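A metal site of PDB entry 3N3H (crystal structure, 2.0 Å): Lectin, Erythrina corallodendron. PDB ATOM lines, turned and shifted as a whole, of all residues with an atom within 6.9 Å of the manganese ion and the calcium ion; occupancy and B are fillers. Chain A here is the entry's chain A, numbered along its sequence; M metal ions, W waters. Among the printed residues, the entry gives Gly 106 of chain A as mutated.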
ATOM      1  N   ASP A  89     -17.056 -32.371  13.333  1.00  0.00           N
ATOM      2  CA  ASP A  89     -17.121 -31.604  14.648  1.00  0.00           C
ATOM      3  C   ASP A  89     -17.884 -32.463  15.601  1.00  0.00           C
ATOM      4  O   ASP A  89     -17.713 -32.397  16.840  1.00  0.00           O
ATOM      5  CB  ASP A  89     -17.831 -30.246  14.505  1.00  0.00           C
ATOM      6  CG  ASP A  89     -16.919 -29.207  14.071  1.00  0.00           C
ATOM      7  OD1 ASP A  89     -16.094 -28.901  14.931  1.00  0.00           O
ATOM      8  OD2 ASP A  89     -16.960 -28.772  12.873  1.00  0.00           O
ATOM      9  N   GLY A  90     -18.762 -33.267  14.980  1.00  0.00           N
ATOM     10  CA  GLY A  90     -19.598 -34.235  15.649  1.00  0.00           C
ATOM     11  C   GLY A  90     -21.087 -34.268  15.302  1.00  0.00           C
ATOM     12  O   GLY A  90     -21.574 -33.681  14.324  1.00  0.00           O
ATOM     13  N   GLY A 106     -20.407 -26.280  12.054  1.00  0.00           N
ATOM     14  CA  GLY A 106     -19.110 -26.439  12.675  1.00  0.00           C
ATOM     15  C   GLY A 106     -19.215 -26.862  14.133  1.00  0.00           C
ATOM     16  O   GLY A 106     -20.000 -27.740  14.481  1.00  0.00           O
ATOM     17  N   GLY A 107     -18.402 -26.236  14.979  1.00  0.00           N
ATOM     18  CA  GLY A 107     -18.396 -26.566  16.402  1.00  0.00           C
ATOM     19  C   GLY A 107     -19.709 -26.344  17.141  1.00  0.00           C
ATOM     20  O   GLY A 107     -19.864 -26.811  18.269  1.00  0.00           O
ATOM     21  N   TYR A 108     -20.647 -25.647  16.516  1.00  0.00           N
ATOM     22  CA  TYR A 108     -21.946 -25.387  17.142  1.00  0.00           C
ATOM     23  C   TYR A 108     -22.931 -26.496  16.849  1.00  0.00           C
ATOM     24  O   TYR A 108     -24.077 -26.484  17.318  1.00  0.00           O
ATOM     25  CB  TYR A 108     -22.483 -24.025  16.689  1.00  0.00           C
ATOM     26  CG  TYR A 108     -21.562 -22.902  17.094  1.00  0.00           C
ATOM     27  CD1 TYR A 108     -21.285 -22.649  18.441  1.00  0.00           C
ATOM     28  CD2 TYR A 108     -20.933 -22.107  16.132  1.00  0.00           C
ATOM     29  CE1 TYR A 108     -20.395 -21.641  18.816  1.00  0.00           C
ATOM     30  CE2 TYR A 108     -20.051 -21.096  16.502  1.00  0.00           C
ATOM     31  CZ  TYR A 108     -19.779 -20.871  17.846  1.00  0.00           C
ATOM     32  OH  TYR A 108     -18.897 -19.882  18.207  1.00  0.00           O
ATOM     33  N   LEU A 109     -22.466 -27.456  16.048  1.00  0.00           N
ATOM     34  CA  LEU A 109     -23.226 -28.654  15.689  1.00  0.00           C
ATOM     35  C   LEU A 109     -24.623 -28.453  15.101  1.00  0.00           C
ATOM     36  O   LEU A 109     -25.424 -29.386  15.101  1.00  0.00           O
ATOM     37  CB  LEU A 109     -23.317 -29.566  16.912  1.00  0.00           C
ATOM     38  CG  LEU A 109     -21.960 -29.908  17.526  1.00  0.00           C
ATOM     39  CD1 LEU A 109     -22.161 -30.734  18.792  1.00  0.00           C
ATOM     40  CD2 LEU A 109     -21.106 -30.665  16.513  1.00  0.00           C
ATOM     41  N   GLU A 127     -24.313 -34.492  23.024  1.00  0.00           N
ATOM     42  CA  GLU A 127     -23.361 -34.507  21.914  1.00  0.00           C
ATOM     43  C   GLU A 127     -22.314 -35.601  21.954  1.00  0.00           C
ATOM     44  O   GLU A 127     -22.049 -36.230  23.001  1.00  0.00           O
ATOM     45  CB  GLU A 127     -22.652 -33.154  21.835  1.00  0.00           C
ATOM     46  CG  GLU A 127     -21.848 -32.888  23.114  1.00  0.00           C
ATOM     47  CD  GLU A 127     -20.924 -31.688  23.050  1.00  0.00           C
ATOM     48  OE1 GLU A 127     -21.322 -30.634  22.561  1.00  0.00           O
ATOM     49  OE2 GLU A 127     -19.777 -31.822  23.468  1.00  0.00           O
ATOM     50  N   PHE A 128     -21.796 -35.839  20.780  1.00  0.00           N
ATOM     51  CA  PHE A 128     -20.724 -36.802  20.567  1.00  0.00           C
ATOM     52  C   PHE A 128     -19.803 -35.918  19.734  1.00  0.00           C
ATOM     53  O   PHE A 128     -19.906 -35.823  18.506  1.00  0.00           O
ATOM     54  CB  PHE A 128     -21.276 -38.002  19.828  1.00  0.00           C
ATOM     55  CG  PHE A 128     -22.309 -38.742  20.622  1.00  0.00           C
ATOM     56  CD1 PHE A 128     -21.923 -39.683  21.569  1.00  0.00           C
ATOM     57  CD2 PHE A 128     -23.647 -38.419  20.500  1.00  0.00           C
ATOM     58  CE1 PHE A 128     -22.872 -40.289  22.395  1.00  0.00           C
ATOM     59  CE2 PHE A 128     -24.607 -39.015  21.327  1.00  0.00           C
ATOM     60  CZ  PHE A 128     -24.207 -39.952  22.275  1.00  0.00           C
ATOM     61  N   ASP A 129     -18.892 -35.239  20.476  1.00  0.00           N
ATOM     62  CA  ASP A 129     -17.970 -34.237  19.963  1.00  0.00           C
ATOM     63  C   ASP A 129     -16.605 -34.746  19.544  1.00  0.00           C
ATOM     64  O   ASP A 129     -15.870 -35.307  20.360  1.00  0.00           O
ATOM     65  CB  ASP A 129     -17.808 -33.198  21.070  1.00  0.00           C
ATOM     66  CG  ASP A 129     -17.349 -31.887  20.553  1.00  0.00           C
ATOM     67  OD1 ASP A 129     -16.658 -31.859  19.526  1.00  0.00           O
ATOM     68  OD2 ASP A 129     -17.677 -30.870  21.199  1.00  0.00           O
ATOM     69  N   THR A 130     -16.282 -34.486  18.268  1.00  0.00           N
ATOM     70  CA  THR A 130     -14.974 -34.992  17.774  1.00  0.00           C
ATOM     71  C   THR A 130     -13.839 -33.982  17.612  1.00  0.00           C
ATOM     72  O   THR A 130     -12.716 -34.362  17.314  1.00  0.00           O
ATOM     73  CB  THR A 130     -15.176 -35.688  16.417  1.00  0.00           C
ATOM     74  OG1 THR A 130     -15.901 -34.821  15.551  1.00  0.00           O
ATOM     75  CG2 THR A 130     -15.954 -36.988  16.577  1.00  0.00           C
ATOM     76  N   PHE A 131     -14.124 -32.691  17.782  1.00  0.00           N
ATOM     77  CA  PHE A 131     -13.093 -31.666  17.632  1.00  0.00           C
ATOM     78  C   PHE A 131     -13.060 -30.784  18.866  1.00  0.00           C
ATOM     79  O   PHE A 131     -14.090 -30.351  19.334  1.00  0.00           O
ATOM     80  CB  PHE A 131     -13.386 -30.776  16.414  1.00  0.00           C
ATOM     81  CG  PHE A 131     -12.363 -29.698  16.188  1.00  0.00           C
ATOM     82  CD1 PHE A 131     -11.197 -29.955  15.468  1.00  0.00           C
ATOM     83  CD2 PHE A 131     -12.527 -28.440  16.756  1.00  0.00           C
ATOM     84  CE1 PHE A 131     -10.218 -28.970  15.307  1.00  0.00           C
ATOM     85  CE2 PHE A 131     -11.560 -27.448  16.614  1.00  0.00           C
ATOM     86  CZ  PHE A 131     -10.404 -27.717  15.886  1.00  0.00           C
ATOM     87  N   SER A 132     -11.871 -30.521  19.412  1.00  0.00           N
ATOM     88  CA  SER A 132     -11.766 -29.705  20.612  1.00  0.00           C
ATOM     89  C   SER A 132     -11.751 -28.188  20.349  1.00  0.00           C
ATOM     90  O   SER A 132     -10.714 -27.638  19.977  1.00  0.00           O
ATOM     91  CB  SER A 132     -10.511 -30.097  21.387  1.00  0.00           C
ATOM     92  OG  SER A 132     -10.436 -29.409  22.620  1.00  0.00           O
ATOM     93  N   ASN A 133     -12.898 -27.526  20.531  1.00  0.00           N
ATOM     94  CA  ASN A 133     -12.960 -26.075  20.336  1.00  0.00           C
ATOM     95  C   ASN A 133     -12.473 -25.381  21.609  1.00  0.00           C
ATOM     96  O   ASN A 133     -12.151 -26.036  22.602  1.00  0.00           O
ATOM     97  CB  ASN A 133     -14.381 -25.603  20.014  1.00  0.00           C
ATOM     98  CG  ASN A 133     -14.876 -26.124  18.689  1.00  0.00           C
ATOM     99  OD1 ASN A 133     -15.407 -27.223  18.605  1.00  0.00           O
ATOM    100  ND2 ASN A 133     -14.709 -25.335  17.634  1.00  0.00           N
ATOM    101  N   GLN A 134     -12.414 -24.056  21.589  1.00  0.00           N
ATOM    102  CA  GLN A 134     -11.944 -23.304  22.745  1.00  0.00           C
ATOM    103  C   GLN A 134     -12.746 -23.513  24.026  1.00  0.00           C
ATOM    104  O   GLN A 134     -12.211 -23.392  25.124  1.00  0.00           O
ATOM    105  CB  GLN A 134     -11.860 -21.820  22.411  1.00  0.00           C
ATOM    106  CG  GLN A 134     -10.859 -21.518  21.304  1.00  0.00           C
ATOM    107  CD  GLN A 134      -9.446 -21.991  21.638  1.00  0.00           C
ATOM    108  OE1 GLN A 134      -8.694 -22.414  20.757  1.00  0.00           O
ATOM    109  NE2 GLN A 134      -9.082 -21.904  22.911  1.00  0.00           N
ATOM    110  N   TRP A 135     -14.027 -23.846  23.884  1.00  0.00           N
ATOM    111  CA  TRP A 135     -14.889 -24.060  25.036  1.00  0.00           C
ATOM    112  C   TRP A 135     -14.937 -25.531  25.465  1.00  0.00           C
ATOM    113  O   TRP A 135     -15.611 -25.880  26.431  1.00  0.00           O
ATOM    114  CB  TRP A 135     -16.312 -23.600  24.694  1.00  0.00           C
ATOM    115  CG  TRP A 135     -16.855 -24.289  23.468  1.00  0.00           C
ATOM    116  CD1 TRP A 135     -17.340 -25.554  23.385  1.00  0.00           C
ATOM    117  CD2 TRP A 135     -16.916 -23.744  22.142  1.00  0.00           C
ATOM    118  NE1 TRP A 135     -17.712 -25.840  22.092  1.00  0.00           N
ATOM    119  CE2 TRP A 135     -17.452 -24.749  21.307  1.00  0.00           C
ATOM    120  CE3 TRP A 135     -16.553 -22.513  21.576  1.00  0.00           C
ATOM    121  CZ2 TRP A 135     -17.651 -24.558  19.931  1.00  0.00           C
ATOM    122  CZ3 TRP A 135     -16.752 -22.322  20.200  1.00  0.00           C
ATOM    123  CH2 TRP A 135     -17.290 -23.344  19.398  1.00  0.00           C
ATOM    124  N   ASP A 136     -14.206 -26.386  24.747  1.00  0.00           N
ATOM    125  CA  ASP A 136     -14.175 -27.825  25.024  1.00  0.00           C
ATOM    126  C   ASP A 136     -13.032 -28.294  25.895  1.00  0.00           C
ATOM    127  O   ASP A 136     -12.027 -27.607  26.053  1.00  0.00           O
ATOM    128  CB  ASP A 136     -14.027 -28.638  23.735  1.00  0.00           C
ATOM    129  CG  ASP A 136     -15.307 -28.747  22.966  1.00  0.00           C
ATOM    130  OD1 ASP A 136     -16.378 -28.836  23.594  1.00  0.00           O
ATOM    131  OD2 ASP A 136     -15.230 -28.768  21.728  1.00  0.00           O
ATOM    132  N   PRO A 137     -13.196 -29.474  26.480  1.00  0.00           N
ATOM    133  CA  PRO A 137     -12.120 -30.022  27.313  1.00  0.00           C
ATOM    134  C   PRO A 137     -11.136 -30.470  26.240  1.00  0.00           C
ATOM    135  O   PRO A 137     -11.511 -30.624  25.065  1.00  0.00           O
ATOM    136  CB  PRO A 137     -12.797 -31.200  28.020  1.00  0.00           C
ATOM    137  CG  PRO A 137     -13.888 -31.610  27.060  1.00  0.00           C
ATOM    138  CD  PRO A 137     -14.425 -30.270  26.616  1.00  0.00           C
ATOM    139  N   VAL A 140     -10.862 -35.487  23.054  1.00  0.00           N
ATOM    140  CA  VAL A 140     -11.857 -35.763  22.039  1.00  0.00           C
ATOM    141  C   VAL A 140     -11.580 -37.167  21.509  1.00  0.00           C
ATOM    142  O   VAL A 140     -10.440 -37.605  21.466  1.00  0.00           O
ATOM    143  CB  VAL A 140     -11.819 -34.752  20.854  1.00  0.00           C
ATOM    144  CG1 VAL A 140     -12.429 -33.433  21.278  1.00  0.00           C
ATOM    145  CG2 VAL A 140     -10.389 -34.552  20.375  1.00  0.00           C
ATOM    146  N   HIS A 142     -15.662 -36.843  22.933  1.00  0.00           N
ATOM    147  CA  HIS A 142     -16.268 -36.894  24.256  1.00  0.00           C
ATOM    148  C   HIS A 142     -17.783 -36.768  24.158  1.00  0.00           C
ATOM    149  O   HIS A 142     -18.314 -36.225  23.191  1.00  0.00           O
ATOM    150  CB  HIS A 142     -15.719 -35.790  25.159  1.00  0.00           C
ATOM    151  CG  HIS A 142     -15.903 -34.392  24.627  1.00  0.00           C
ATOM    152  ND1 HIS A 142     -14.902 -33.706  23.983  1.00  0.00           N
ATOM    153  CD2 HIS A 142     -16.984 -33.577  24.627  1.00  0.00           C
ATOM    154  CE1 HIS A 142     -15.348 -32.519  23.606  1.00  0.00           C
ATOM    155  NE2 HIS A 142     -16.613 -32.420  23.990  1.00  0.00           N
ATOM    156  N   ILE A 143     -18.460 -37.313  25.150  1.00  0.00           N
ATOM    157  CA  ILE A 143     -19.910 -37.222  25.212  1.00  0.00           C
ATOM    158  C   ILE A 143     -20.118 -35.988  26.079  1.00  0.00           C
ATOM    159  O   ILE A 143     -19.362 -35.750  27.012  1.00  0.00           O
ATOM    160  CB  ILE A 143     -20.544 -38.417  25.941  1.00  0.00           C
ATOM    161  CG1 ILE A 143     -20.099 -39.727  25.278  1.00  0.00           C
ATOM    162  CG2 ILE A 143     -22.060 -38.277  25.919  1.00  0.00           C
ATOM    163  CD1 ILE A 143     -20.449 -40.962  26.070  1.00  0.00           C
ATOM    164  N   GLY A 144     -21.143 -35.200  25.764  1.00  0.00           N
ATOM    165  CA  GLY A 144     -21.394 -34.024  26.566  1.00  0.00           C
ATOM    166  C   GLY A 144     -22.871 -33.773  26.737  1.00  0.00           C
ATOM    167  O   GLY A 144     -23.657 -34.097  25.853  1.00  0.00           O
ATOM    168  N   ASP A 146     -25.423 -30.887  26.990  1.00  0.00           N
ATOM    169  CA  ASP A 146     -25.512 -29.453  26.724  1.00  0.00           C
ATOM    170  C   ASP A 146     -26.855 -28.883  27.132  1.00  0.00           C
ATOM    171  O   ASP A 146     -27.905 -29.329  26.662  1.00  0.00           O
ATOM    172  CB  ASP A 146     -25.273 -29.166  25.242  1.00  0.00           C
ATOM    173  CG  ASP A 146     -23.943 -29.710  24.737  1.00  0.00           C
ATOM    174  OD1 ASP A 146     -23.050 -29.989  25.567  1.00  0.00           O
ATOM    175  OD2 ASP A 146     -23.780 -29.839  23.502  1.00  0.00           O
ATOM    176  N   ILE A 150     -23.265 -24.577  24.192  1.00  0.00           N
ATOM    177  CA  ILE A 150     -22.406 -25.562  23.550  1.00  0.00           C
ATOM    178  C   ILE A 150     -21.338 -25.989  24.558  1.00  0.00           C
ATOM    179  O   ILE A 150     -20.682 -27.019  24.396  1.00  0.00           O
ATOM    180  CB  ILE A 150     -21.741 -24.963  22.278  1.00  0.00           C
ATOM    181  CG1 ILE A 150     -21.019 -26.070  21.506  1.00  0.00           C
ATOM    182  CG2 ILE A 150     -20.782 -23.838  22.666  1.00  0.00           C
ATOM    183  CD1 ILE A 150     -21.956 -27.127  20.916  1.00  0.00           C
ATOM    184  N   ARG A 151     -21.183 -25.188  25.611  1.00  0.00           N
ATOM    185  CA  ARG A 151     -20.228 -25.502  26.676  1.00  0.00           C
ATOM    186  C   ARG A 151     -20.975 -26.443  27.632  1.00  0.00           C
ATOM    187  O   ARG A 151     -21.805 -26.006  28.433  1.00  0.00           O
ATOM    188  CB  ARG A 151     -19.791 -24.216  27.393  1.00  0.00           C
ATOM    189  CG  ARG A 151     -18.785 -24.451  28.519  1.00  0.00           C
ATOM    190  CD  ARG A 151     -18.343 -23.156  29.214  1.00  0.00           C
ATOM    191  NE  ARG A 151     -17.245 -22.481  28.518  1.00  0.00           N
ATOM    192  CZ  ARG A 151     -17.392 -21.571  27.559  1.00  0.00           C
ATOM    193  NH1 ARG A 151     -18.601 -21.212  27.164  1.00  0.00           N
ATOM    194  NH2 ARG A 151     -16.314 -21.023  27.007  1.00  0.00           N
ATOM    195  N   SER A 152     -20.668 -27.724  27.540  1.00  0.00           N
ATOM    196  CA  SER A 152     -21.317 -28.766  28.342  1.00  0.00           C
ATOM    197  C   SER A 152     -21.215 -28.595  29.853  1.00  0.00           C
ATOM    198  O   SER A 152     -20.199 -28.128  30.377  1.00  0.00           O
ATOM    199  CB  SER A 152     -20.736 -30.137  27.977  1.00  0.00           C
ATOM    200  OG  SER A 152     -20.714 -30.311  26.572  1.00  0.00           O
ATOM    201  N   THR A 155     -18.948 -33.652  30.755  1.00  0.00           N
ATOM    202  CA  THR A 155     -18.421 -34.407  29.621  1.00  0.00           C
ATOM    203  C   THR A 155     -17.789 -35.719  30.063  1.00  0.00           C
ATOM    204  O   THR A 155     -17.422 -35.887  31.229  1.00  0.00           O
ATOM    205  CB  THR A 155     -17.352 -33.604  28.852  1.00  0.00           C
ATOM    206  OG1 THR A 155     -16.260 -33.287  29.727  1.00  0.00           O
ATOM    207  CG2 THR A 155     -17.942 -32.308  28.292  1.00  0.00           C
HETATM  208 MN    MN M   1     -17.932 -30.578  23.374  1.00  0.00          MN
HETATM  209 CA    CA M   2     -16.317 -29.341  19.637  1.00  0.00          CA
HETATM  210  O   HOH W   1     -18.258 -29.974  25.701  1.00  0.00           O
HETATM  211  O   HOH W   2     -19.514 -28.776  22.727  1.00  0.00           O
HETATM  212  O   HOH W   3     -16.981 -29.900  17.291  1.00  0.00           O
HETATM  213  O   HOH W   4     -18.523 -28.188  20.135  1.00  0.00           O
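The side-chain carboxylate (OD2) of Asp 146 lies close to the side-chain carboxylate (OE1) of Glu 127 (2.7 Å).
N of Glu 127 sits at hydrogen-bond distance from O of Gly 144, at 2.9 Å.
Within 4 Å of the manganese ion: Glu 127, Asp 129, Asp 136 and His 142.
Along chain A the residues within 4 Å of the manganese ion span positions 127 to 142.
Four residues have an atom within 4 Å of the calcium ion: Asp 129, Phe 131, Asn 133 and Asp 136.
Along chain A the residues within 4 Å of the calcium ion span positions 129 to 136.
The nearest printed residue that does not touch the calcium ion is Asp 89 (4.4 Å).
The manganese ion is bound by OD2 of Asp 129 (2.2 Å), OE2 of Glu 127 (2.2 Å), OD1 of Asp 136 (2.3 Å), NE2 of His 142 (2.3 Å), water W1 (2.4 Å) and water W2 (2.5 Å).
The calcium ion is bound by the side-chain carboxylate (OD2) of Asp 136, the backbone carbonyl oxygen (O) of Phe 131, water W3, the side-chain amide oxygen (OD1) of Asn 133, water W4, the side-chain carboxylate (OD1) of Asp 129 and the side-chain carboxylate (OD2) of Asp 129.
The calcium ion has seven donor atoms within binding distance.
Water W2 bridges OE1 of Glu 127 (2.6 Å) and O of Ile 150 (2.7 Å).
Water W4 bridges the backbone carbonyl oxygen (O) of Gly 107 and the indole nitrogen (NE1) of Trp 135.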
